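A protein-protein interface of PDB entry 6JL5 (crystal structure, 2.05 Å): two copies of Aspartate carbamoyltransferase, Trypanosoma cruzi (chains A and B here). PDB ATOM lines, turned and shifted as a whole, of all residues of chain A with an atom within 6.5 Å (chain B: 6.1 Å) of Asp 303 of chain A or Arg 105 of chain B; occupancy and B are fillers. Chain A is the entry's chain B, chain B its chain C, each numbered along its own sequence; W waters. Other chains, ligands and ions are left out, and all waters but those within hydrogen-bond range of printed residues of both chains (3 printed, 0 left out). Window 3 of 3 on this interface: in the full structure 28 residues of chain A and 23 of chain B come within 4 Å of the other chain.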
ATOM      1  N   ARG A 294      -5.607  26.381 -19.829  1.00  0.00           N
ATOM      2  CA  ARG A 294      -5.604  24.924 -19.854  1.00  0.00           C
ATOM      3  C   ARG A 294      -6.191  24.306 -18.572  1.00  0.00           C
ATOM      4  O   ARG A 294      -6.157  24.910 -17.490  1.00  0.00           O
ATOM      5  CB  ARG A 294      -4.178  24.378 -20.061  1.00  0.00           C
ATOM      6  CG  ARG A 294      -3.151  24.937 -19.051  1.00  0.00           C
ATOM      7  CD  ARG A 294      -1.844  24.180 -19.017  1.00  0.00           C
ATOM      8  NE  ARG A 294      -0.872  24.894 -18.180  1.00  0.00           N
ATOM      9  CZ  ARG A 294       0.371  24.498 -17.937  1.00  0.00           C
ATOM     10  NH1 ARG A 294       0.823  23.338 -18.418  1.00  0.00           N
ATOM     11  NH2 ARG A 294       1.162  25.269 -17.186  1.00  0.00           N
ATOM     12  N   LEU A 298      -3.114  19.324 -20.607  1.00  0.00           N
ATOM     13  CA  LEU A 298      -1.740  19.754 -20.848  1.00  0.00           C
ATOM     14  C   LEU A 298      -1.002  19.880 -19.521  1.00  0.00           C
ATOM     15  O   LEU A 298      -1.150  20.870 -18.826  1.00  0.00           O
ATOM     16  CB  LEU A 298      -1.683  21.060 -21.686  1.00  0.00           C
ATOM     17  CG  LEU A 298      -0.281  21.673 -21.973  1.00  0.00           C
ATOM     18  CD1 LEU A 298       0.677  20.656 -22.627  1.00  0.00           C
ATOM     19  CD2 LEU A 298      -0.445  22.868 -22.863  1.00  0.00           C
ATOM     20  N   SER A 299      -0.219  18.850 -19.200  1.00  0.00           N
ATOM     21  CA  SER A 299       0.416  18.672 -17.888  1.00  0.00           C
ATOM     22  C   SER A 299       1.505  19.720 -17.638  1.00  0.00           C
ATOM     23  O   SER A 299       2.256  20.065 -18.552  1.00  0.00           O
ATOM     24  CB  SER A 299       1.016  17.261 -17.782  1.00  0.00           C
ATOM     25  OG  SER A 299       1.952  17.147 -16.705  1.00  0.00           O
ATOM     26  N   THR A 300       1.608  20.209 -16.401  1.00  0.00           N
ATOM     27  CA  THR A 300       2.695  21.125 -16.059  1.00  0.00           C
ATOM     28  C   THR A 300       4.084  20.489 -16.227  1.00  0.00           C
ATOM     29  O   THR A 300       5.081  21.215 -16.210  1.00  0.00           O
ATOM     30  CB  THR A 300       2.569  21.650 -14.623  1.00  0.00           C
ATOM     31  OG1 THR A 300       2.627  20.536 -13.730  1.00  0.00           O
ATOM     32  CG2 THR A 300       1.225  22.409 -14.418  1.00  0.00           C
ATOM     33  N   THR A 301       4.160  19.156 -16.386  1.00  0.00           N
ATOM     34  CA  THR A 301       5.445  18.470 -16.643  1.00  0.00           C
ATOM     35  C   THR A 301       6.070  18.769 -18.008  1.00  0.00           C
ATOM     36  O   THR A 301       7.210  18.368 -18.269  1.00  0.00           O
ATOM     37  CB  THR A 301       5.340  16.935 -16.582  1.00  0.00           C
ATOM     38  OG1 THR A 301       4.336  16.490 -17.513  1.00  0.00           O
ATOM     39  CG2 THR A 301       5.022  16.427 -15.128  1.00  0.00           C
ATOM     40  N   VAL A 302       5.312  19.415 -18.888  1.00  0.00           N
ATOM     41  CA  VAL A 302       5.769  19.731 -20.244  1.00  0.00           C
ATOM     42  C   VAL A 302       6.352  21.152 -20.238  1.00  0.00           C
ATOM     43  O   VAL A 302       7.094  21.533 -21.149  1.00  0.00           O
ATOM     44  CB  VAL A 302       4.586  19.663 -21.260  1.00  0.00           C
ATOM     45  CG1 VAL A 302       4.982  20.141 -22.682  1.00  0.00           C
ATOM     46  CG2 VAL A 302       3.976  18.248 -21.310  1.00  0.00           C
ATOM     47  N   ASP A 303       6.011  21.935 -19.211  1.00  0.00           N
ATOM     48  CA  ASP A 303       6.339  23.377 -19.215  1.00  0.00           C
ATOM     49  C   ASP A 303       7.827  23.688 -19.359  1.00  0.00           C
ATOM     50  O   ASP A 303       8.169  24.722 -19.925  1.00  0.00           O
ATOM     51  CB  ASP A 303       5.804  24.091 -17.969  1.00  0.00           C
ATOM     52  CG  ASP A 303       4.314  24.043 -17.865  1.00  0.00           C
ATOM     53  OD1 ASP A 303       3.643  23.553 -18.805  1.00  0.00           O
ATOM     54  OD2 ASP A 303       3.805  24.483 -16.819  1.00  0.00           O
ATOM     55  N   ALA A 304       8.702  22.811 -18.860  1.00  0.00           N
ATOM     56  CA  ALA A 304      10.162  23.055 -18.947  1.00  0.00           C
ATOM     57  C   ALA A 304      10.729  22.661 -20.303  1.00  0.00           C
ATOM     58  O   ALA A 304      11.848  23.037 -20.632  1.00  0.00           O
ATOM     59  CB  ALA A 304      10.924  22.323 -17.817  1.00  0.00           C
ATOM     60  N   ASP A 305       9.961  21.894 -21.081  1.00  0.00           N
ATOM     61  CA  ASP A 305      10.383  21.459 -22.394  1.00  0.00           C
ATOM     62  C   ASP A 305      10.534  22.681 -23.298  1.00  0.00           C
ATOM     63  O   ASP A 305       9.612  23.500 -23.414  1.00  0.00           O
ATOM     64  CB  ASP A 305       9.354  20.487 -22.990  1.00  0.00           C
ATOM     65  CG  ASP A 305       9.950  19.577 -24.067  1.00  0.00           C
ATOM     66  OD1 ASP A 305      10.558  20.081 -25.039  1.00  0.00           O
ATOM     67  OD2 ASP A 305       9.799  18.341 -23.943  1.00  0.00           O
ATOM     68  N   PRO A 306      11.689  22.804 -23.962  1.00  0.00           N
ATOM     69  CA  PRO A 306      11.890  23.860 -24.972  1.00  0.00           C
ATOM     70  C   PRO A 306      10.831  23.851 -26.109  1.00  0.00           C
ATOM     71  O   PRO A 306      10.593  24.884 -26.741  1.00  0.00           O
ATOM     72  CB  PRO A 306      13.287  23.541 -25.527  1.00  0.00           C
ATOM     73  CG  PRO A 306      13.555  22.121 -25.113  1.00  0.00           C
ATOM     74  CD  PRO A 306      12.872  21.937 -23.819  1.00  0.00           C
ATOM     75  N   ALA A 308       7.677  23.359 -25.602  1.00  0.00           N
ATOM     76  CA  ALA A 308       6.497  24.011 -25.033  1.00  0.00           C
ATOM     77  C   ALA A 308       6.441  25.480 -25.491  1.00  0.00           C
ATOM     78  O   ALA A 308       7.145  26.323 -24.930  1.00  0.00           O
ATOM     79  CB  ALA A 308       6.525  23.937 -23.504  1.00  0.00           C
ATOM     80  N   TYR A 310       3.473  27.360 -25.579  1.00  0.00           N
ATOM     81  CA  TYR A 310       2.176  27.984 -25.218  1.00  0.00           C
ATOM     82  C   TYR A 310       2.282  29.227 -24.343  1.00  0.00           C
ATOM     83  O   TYR A 310       1.307  30.012 -24.273  1.00  0.00           O
ATOM     84  CB  TYR A 310       1.175  26.960 -24.636  1.00  0.00           C
ATOM     85  CG  TYR A 310       1.812  25.910 -23.767  1.00  0.00           C
ATOM     86  CD1 TYR A 310       1.918  26.087 -22.383  1.00  0.00           C
ATOM     87  CD2 TYR A 310       2.341  24.744 -24.333  1.00  0.00           C
ATOM     88  CE1 TYR A 310       2.496  25.101 -21.585  1.00  0.00           C
ATOM     89  CE2 TYR A 310       2.952  23.768 -23.547  1.00  0.00           C
ATOM     90  CZ  TYR A 310       3.020  23.944 -22.174  1.00  0.00           C
ATOM     91  OH  TYR A 310       3.624  22.956 -21.383  1.00  0.00           O
ATOM     92  N   PHE A 311       3.441  29.440 -23.704  1.00  0.00           N
ATOM     93  CA  PHE A 311       3.660  30.708 -23.020  1.00  0.00           C
ATOM     94  C   PHE A 311       4.170  31.790 -23.951  1.00  0.00           C
ATOM     95  O   PHE A 311       3.650  32.899 -23.943  1.00  0.00           O
ATOM     96  CB  PHE A 311       4.531  30.538 -21.770  1.00  0.00           C
ATOM     97  CG  PHE A 311       3.988  29.502 -20.819  1.00  0.00           C
ATOM     98  CD1 PHE A 311       2.664  29.586 -20.368  1.00  0.00           C
ATOM     99  CD2 PHE A 311       4.783  28.434 -20.385  1.00  0.00           C
ATOM    100  CE1 PHE A 311       2.159  28.637 -19.490  1.00  0.00           C
ATOM    101  CE2 PHE A 311       4.271  27.483 -19.503  1.00  0.00           C
ATOM    102  CZ  PHE A 311       2.953  27.594 -19.066  1.00  0.00           C
ATOM    103  N   MET A 314       1.448  33.543 -26.069  1.00  0.00           N
ATOM    104  CA  MET A 314       0.771  34.753 -25.572  1.00  0.00           C
ATOM    105  C   MET A 314       1.490  36.074 -25.930  1.00  0.00           C
ATOM    106  O   MET A 314       0.834  37.091 -26.200  1.00  0.00           O
ATOM    107  CB  MET A 314       0.556  34.662 -24.068  1.00  0.00           C
ATOM    108  CG  MET A 314      -0.435  33.561 -23.678  1.00  0.00           C
ATOM    109  SD  MET A 314      -0.801  33.642 -21.922  1.00  0.00           S
ATOM    110  CE  MET A 314       0.624  32.733 -21.239  1.00  0.00           C
ATOM    111  N   THR B  99      -4.769  28.182 -13.222  1.00  0.00           N
ATOM    112  CA  THR B  99      -3.986  28.249 -11.959  1.00  0.00           C
ATOM    113  C   THR B  99      -3.323  29.630 -11.725  1.00  0.00           C
ATOM    114  O   THR B  99      -3.176  30.442 -12.662  1.00  0.00           O
ATOM    115  CB  THR B  99      -2.831  27.183 -11.937  1.00  0.00           C
ATOM    116  OG1 THR B  99      -1.866  27.485 -12.961  1.00  0.00           O
ATOM    117  CG2 THR B  99      -3.379  25.736 -12.160  1.00  0.00           C
ATOM    118  N   LEU B 100      -2.911  29.882 -10.479  1.00  0.00           N
ATOM    119  CA  LEU B 100      -2.209  31.109 -10.139  1.00  0.00           C
ATOM    120  C   LEU B 100      -0.943  31.285 -10.982  1.00  0.00           C
ATOM    121  O   LEU B 100      -0.733  32.364 -11.544  1.00  0.00           O
ATOM    122  CB  LEU B 100      -1.856  31.168  -8.656  1.00  0.00           C
ATOM    123  CG  LEU B 100      -0.897  32.325  -8.294  1.00  0.00           C
ATOM    124  CD1 LEU B 100      -1.582  33.689  -8.429  1.00  0.00           C
ATOM    125  CD2 LEU B 100      -0.345  32.140  -6.888  1.00  0.00           C
ATOM    126  N   ALA B 101      -0.114  30.238 -11.075  1.00  0.00           N
ATOM    127  CA  ALA B 101       1.080  30.269 -11.921  1.00  0.00           C
ATOM    128  C   ALA B 101       0.785  30.662 -13.369  1.00  0.00           C
ATOM    129  O   ALA B 101       1.473  31.513 -13.926  1.00  0.00           O
ATOM    130  CB  ALA B 101       1.849  28.942 -11.872  1.00  0.00           C
ATOM    131  N   ASP B 102      -0.223  30.034 -13.976  1.00  0.00           N
ATOM    132  CA  ASP B 102      -0.575  30.327 -15.359  1.00  0.00           C
ATOM    133  C   ASP B 102      -1.070  31.768 -15.490  1.00  0.00           C
ATOM    134  O   ASP B 102      -0.738  32.451 -16.454  1.00  0.00           O
ATOM    135  CB  ASP B 102      -1.632  29.340 -15.907  1.00  0.00           C
ATOM    136  CG  ASP B 102      -1.037  28.010 -16.354  1.00  0.00           C
ATOM    137  OD1 ASP B 102       0.203  27.856 -16.301  1.00  0.00           O
ATOM    138  OD2 ASP B 102      -1.819  27.104 -16.766  1.00  0.00           O
ATOM    139  N   THR B 103      -1.851  32.227 -14.512  1.00  0.00           N
ATOM    140  CA  THR B 103      -2.269  33.641 -14.423  1.00  0.00           C
ATOM    141  C   THR B 103      -1.054  34.603 -14.397  1.00  0.00           C
ATOM    142  O   THR B 103      -0.992  35.553 -15.202  1.00  0.00           O
ATOM    143  CB  THR B 103      -3.219  33.843 -13.222  1.00  0.00           C
ATOM    144  OG1 THR B 103      -4.405  33.075 -13.447  1.00  0.00           O
ATOM    145  CG2 THR B 103      -3.627  35.324 -13.038  1.00  0.00           C
ATOM    146  N   ILE B 104      -0.079  34.326 -13.525  1.00  0.00           N
ATOM    147  CA  ILE B 104       1.175  35.077 -13.496  1.00  0.00           C
ATOM    148  C   ILE B 104       1.898  35.100 -14.864  1.00  0.00           C
ATOM    149  O   ILE B 104       2.233  36.163 -15.354  1.00  0.00           O
ATOM    150  CB  ILE B 104       2.171  34.547 -12.427  1.00  0.00           C
ATOM    151  CG1 ILE B 104       1.667  34.793 -11.018  1.00  0.00           C
ATOM    152  CG2 ILE B 104       3.576  35.204 -12.612  1.00  0.00           C
ATOM    153  CD1 ILE B 104       1.536  36.267 -10.663  1.00  0.00           C
ATOM    154  N   ARG B 105       2.150  33.931 -15.453  1.00  0.00           N
ATOM    155  CA  ARG B 105       2.735  33.856 -16.789  1.00  0.00           C
ATOM    156  C   ARG B 105       1.932  34.671 -17.790  1.00  0.00           C
ATOM    157  O   ARG B 105       2.507  35.308 -18.666  1.00  0.00           O
ATOM    158  CB  ARG B 105       2.877  32.420 -17.278  1.00  0.00           C
ATOM    159  CG  ARG B 105       3.932  31.591 -16.532  1.00  0.00           C
ATOM    160  CD  ARG B 105       3.824  30.136 -16.944  1.00  0.00           C
ATOM    161  NE  ARG B 105       4.748  29.227 -16.274  1.00  0.00           N
ATOM    162  CZ  ARG B 105       4.358  28.204 -15.507  1.00  0.00           C
ATOM    163  NH1 ARG B 105       3.052  27.971 -15.275  1.00  0.00           N
ATOM    164  NH2 ARG B 105       5.271  27.402 -14.969  1.00  0.00           N
ATOM    165  N   THR B 106       0.609  34.676 -17.650  1.00  0.00           N
ATOM    166  CA  THR B 106      -0.222  35.436 -18.569  1.00  0.00           C
ATOM    167  C   THR B 106       0.069  36.956 -18.481  1.00  0.00           C
ATOM    168  O   THR B 106       0.434  37.549 -19.491  1.00  0.00           O
ATOM    169  CB  THR B 106      -1.702  35.111 -18.426  1.00  0.00           C
ATOM    170  OG1 THR B 106      -1.911  33.716 -18.702  1.00  0.00           O
ATOM    171  CG2 THR B 106      -2.511  35.895 -19.440  1.00  0.00           C
ATOM    172  N   LEU B 107      -0.102  37.581 -17.309  1.00  0.00           N
ATOM    173  CA  LEU B 107       0.172  39.032 -17.154  1.00  0.00           C
ATOM    174  C   LEU B 107       1.623  39.364 -17.476  1.00  0.00           C
ATOM    175  O   LEU B 107       1.951  40.429 -18.003  1.00  0.00           O
ATOM    176  CB  LEU B 107      -0.161  39.516 -15.732  1.00  0.00           C
ATOM    177  CG  LEU B 107      -1.651  39.780 -15.484  1.00  0.00           C
ATOM    178  CD1 LEU B 107      -2.553  38.690 -15.995  1.00  0.00           C
ATOM    179  CD2 LEU B 107      -1.854  39.997 -13.975  1.00  0.00           C
ATOM    180  N   ASP B 108       2.489  38.406 -17.216  1.00  0.00           N
ATOM    181  CA  ASP B 108       3.909  38.535 -17.510  1.00  0.00           C
ATOM    182  C   ASP B 108       4.258  38.677 -18.988  1.00  0.00           C
ATOM    183  O   ASP B 108       5.282  39.273 -19.333  1.00  0.00           O
ATOM    184  CB  ASP B 108       4.612  37.319 -16.946  1.00  0.00           C
ATOM    185  CG  ASP B 108       6.012  37.600 -16.498  1.00  0.00           C
ATOM    186  OD1 ASP B 108       6.300  38.658 -15.894  1.00  0.00           O
ATOM    187  OD2 ASP B 108       6.820  36.699 -16.732  1.00  0.00           O
ATOM    188  N   SER B 109       3.408  38.143 -19.871  1.00  0.00           N
ATOM    189  CA  SER B 109       3.644  38.236 -21.310  1.00  0.00           C
ATOM    190  C   SER B 109       3.518  39.662 -21.877  1.00  0.00           C
ATOM    191  O   SER B 109       4.007  39.926 -22.984  1.00  0.00           O
ATOM    192  CB  SER B 109       2.617  37.375 -22.031  1.00  0.00           C
ATOM    193  OG  SER B 109       2.466  36.171 -21.328  1.00  0.00           O
ATOM    194  N   TYR B 110       2.845  40.555 -21.156  1.00  0.00           N
ATOM    195  CA  TYR B 110       2.444  41.868 -21.672  1.00  0.00           C
ATOM    196  C   TYR B 110       2.956  43.040 -20.835  1.00  0.00           C
ATOM    197  O   TYR B 110       2.939  44.172 -21.296  1.00  0.00           O
ATOM    198  CB  TYR B 110       0.909  41.983 -21.697  1.00  0.00           C
ATOM    199  CG  TYR B 110       0.159  40.750 -22.144  1.00  0.00           C
ATOM    200  CD1 TYR B 110       0.396  40.179 -23.391  1.00  0.00           C
ATOM    201  CD2 TYR B 110      -0.819  40.184 -21.333  1.00  0.00           C
ATOM    202  CE1 TYR B 110      -0.301  39.076 -23.813  1.00  0.00           C
ATOM    203  CE2 TYR B 110      -1.531  39.067 -21.751  1.00  0.00           C
ATOM    204  CZ  TYR B 110      -1.255  38.526 -22.988  1.00  0.00           C
ATOM    205  OH  TYR B 110      -1.934  37.427 -23.381  1.00  0.00           O
ATOM    206  N   VAL B 130       7.866  31.875 -11.236  1.00  0.00           N
ATOM    207  CA  VAL B 130       7.539  31.825 -12.672  1.00  0.00           C
ATOM    208  C   VAL B 130       7.632  33.170 -13.426  1.00  0.00           C
ATOM    209  O   VAL B 130       7.771  33.167 -14.625  1.00  0.00           O
ATOM    210  CB  VAL B 130       6.168  31.098 -13.004  1.00  0.00           C
ATOM    211  CG1 VAL B 130       6.118  29.715 -12.364  1.00  0.00           C
ATOM    212  CG2 VAL B 130       4.986  31.928 -12.557  1.00  0.00           C
ATOM    213  N   ALA B 131       7.586  34.303 -12.729  1.00  0.00           N
ATOM    214  CA  ALA B 131       7.588  35.615 -13.417  1.00  0.00           C
ATOM    215  C   ALA B 131       8.977  36.032 -13.889  1.00  0.00           C
ATOM    216  O   ALA B 131       9.967  35.849 -13.165  1.00  0.00           O
ATOM    217  CB  ALA B 131       6.986  36.717 -12.527  1.00  0.00           C
HETATM  218  O   HOH W   1      -4.218  26.396 -15.463  1.00  0.00           O
HETATM  219  O   HOH W   2      -1.851  37.354 -25.982  1.00  0.00           O
HETATM  220  O   HOH W   3      -3.951  28.103 -18.227  1.00  0.00           O
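No position is printed for both chains.
Of the 8 pairs that touch across the chains among the printed residues, none has its exchanged pair printed and touching as well.
Water W2 bridges OH of Tyr 110 of chain B and O of Met 314 of chain A.
Water W3 bridges the side-chain carboxylate of Asp 102 of chain B and the backbone NH of Arg 294 of chain A.
Water W1 lies within hydrogen-bond range of the side-chain carboxylate of Asp 102 of chain B, the backbone NH of Thr 99 of chain B and the backbone carbonyl oxygen of Arg 294 of chain A.
Of chain B, only Arg 105 comes within 4 Å of Asp 303 of chain A.
Arg 105 of chain B touches three residues of chain A.
Of the printed residues of chain B, Phe 311 of chain A touches Asp 102 (3.8 Å) and Arg 105 (3.4 Å).
Printed residues of chain B within 4 Å of Met 314 of chain A: Thr 106, Ser 109 and Tyr 110.
Of the printed residues of chain A, Asp 102 of chain B touches Arg 294 and Phe 311.
Asp 108 of chain B touches none of the printed residues of chain A.
Ala 101 of chain B touches none of the printed residues of chain A.
The nearest residue of chain B that does not touch Asp 303 of chain A is Asp 102 of chain B (5.0 Å).
The nearest residue of chain A that does not touch Arg 105 of chain B is Met 314 of chain A (4.1 Å).
The nearest printed residue of chain B that does not touch Arg 294 of chain A is Thr 99 of chain B (5.6 Å).
The side-chain carboxylate (OD2) of Asp 102 of chain B is in salt-bridge range of the guanidinium group (NE) of Arg 294 of chain A.
The guanidinium group (NH2) of Arg 105 of chain B is in salt-bridge range of the side-chain carboxylate (OD2) of Asp 303 of chain A, at 3.8 Å.
The side-chain sulfur (SD) of Met 314 of chain A is in hydrogen-bond range of the side-chain hydroxyl (OG1) of Thr 106 of chain B, at 3.4 Å.
NH2 of Arg 294 of chain A touches NH1 of Arg 105 of chain B, at 3.8 Å.
Phe 311 of chain A touches Asp 102 of chain B (CE1 to OD1, 3.8 Å).
Phe 311 of chain A touches Arg 105 of chain B.
Ser 109 of chain B touches Met 314 of chain A.
Met 314 of chain A touches Tyr 110 of chain B.
Printed residues of chain A that touch a printed residue of chain B: Arg 294, Asp 303, Phe 311 and Met 314.
Of the 14 printed residues of chain B, 5 touch a printed residue of chain A.
Hydrophobic or aromatic side chains of chain B within 4 Å of the printed part of chain A: Tyr 110.
Along chain B the printed residues that touch a printed residue of chain A span positions 102 to 110.
Among the printed residues, 8 pairs touch across the chains.
O of Leu 298 of chain A is in hydrogen-bond range of NH1 of Arg 294 of chain A (3.2 Å).
OD2 of Asp 303 of chain A lies within salt-bridge range of NH2 of Arg 294 of chain A (2.8 Å).
The side-chain hydroxyl (OG1) of Thr 99 of chain B lies within hydrogen-bond range of the backbone NH (N) of Asp 102 of chain B (3.2 Å).
The guanidinium group (NH1) of Arg 105 of chain B lies within salt-bridge range of the side-chain carboxylate (OD1) of Asp 102 of chain B (3.0 Å).
O of Arg 105 of chain B sits at hydrogen-bond distance from OG of Ser 109 of chain B.
The side-chain hydroxyl (OG) of Ser 109 of chain B sits at hydrogen-bond distance from the backbone carbonyl oxygen (O) of Thr 106 of chain B (3.1 Å).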
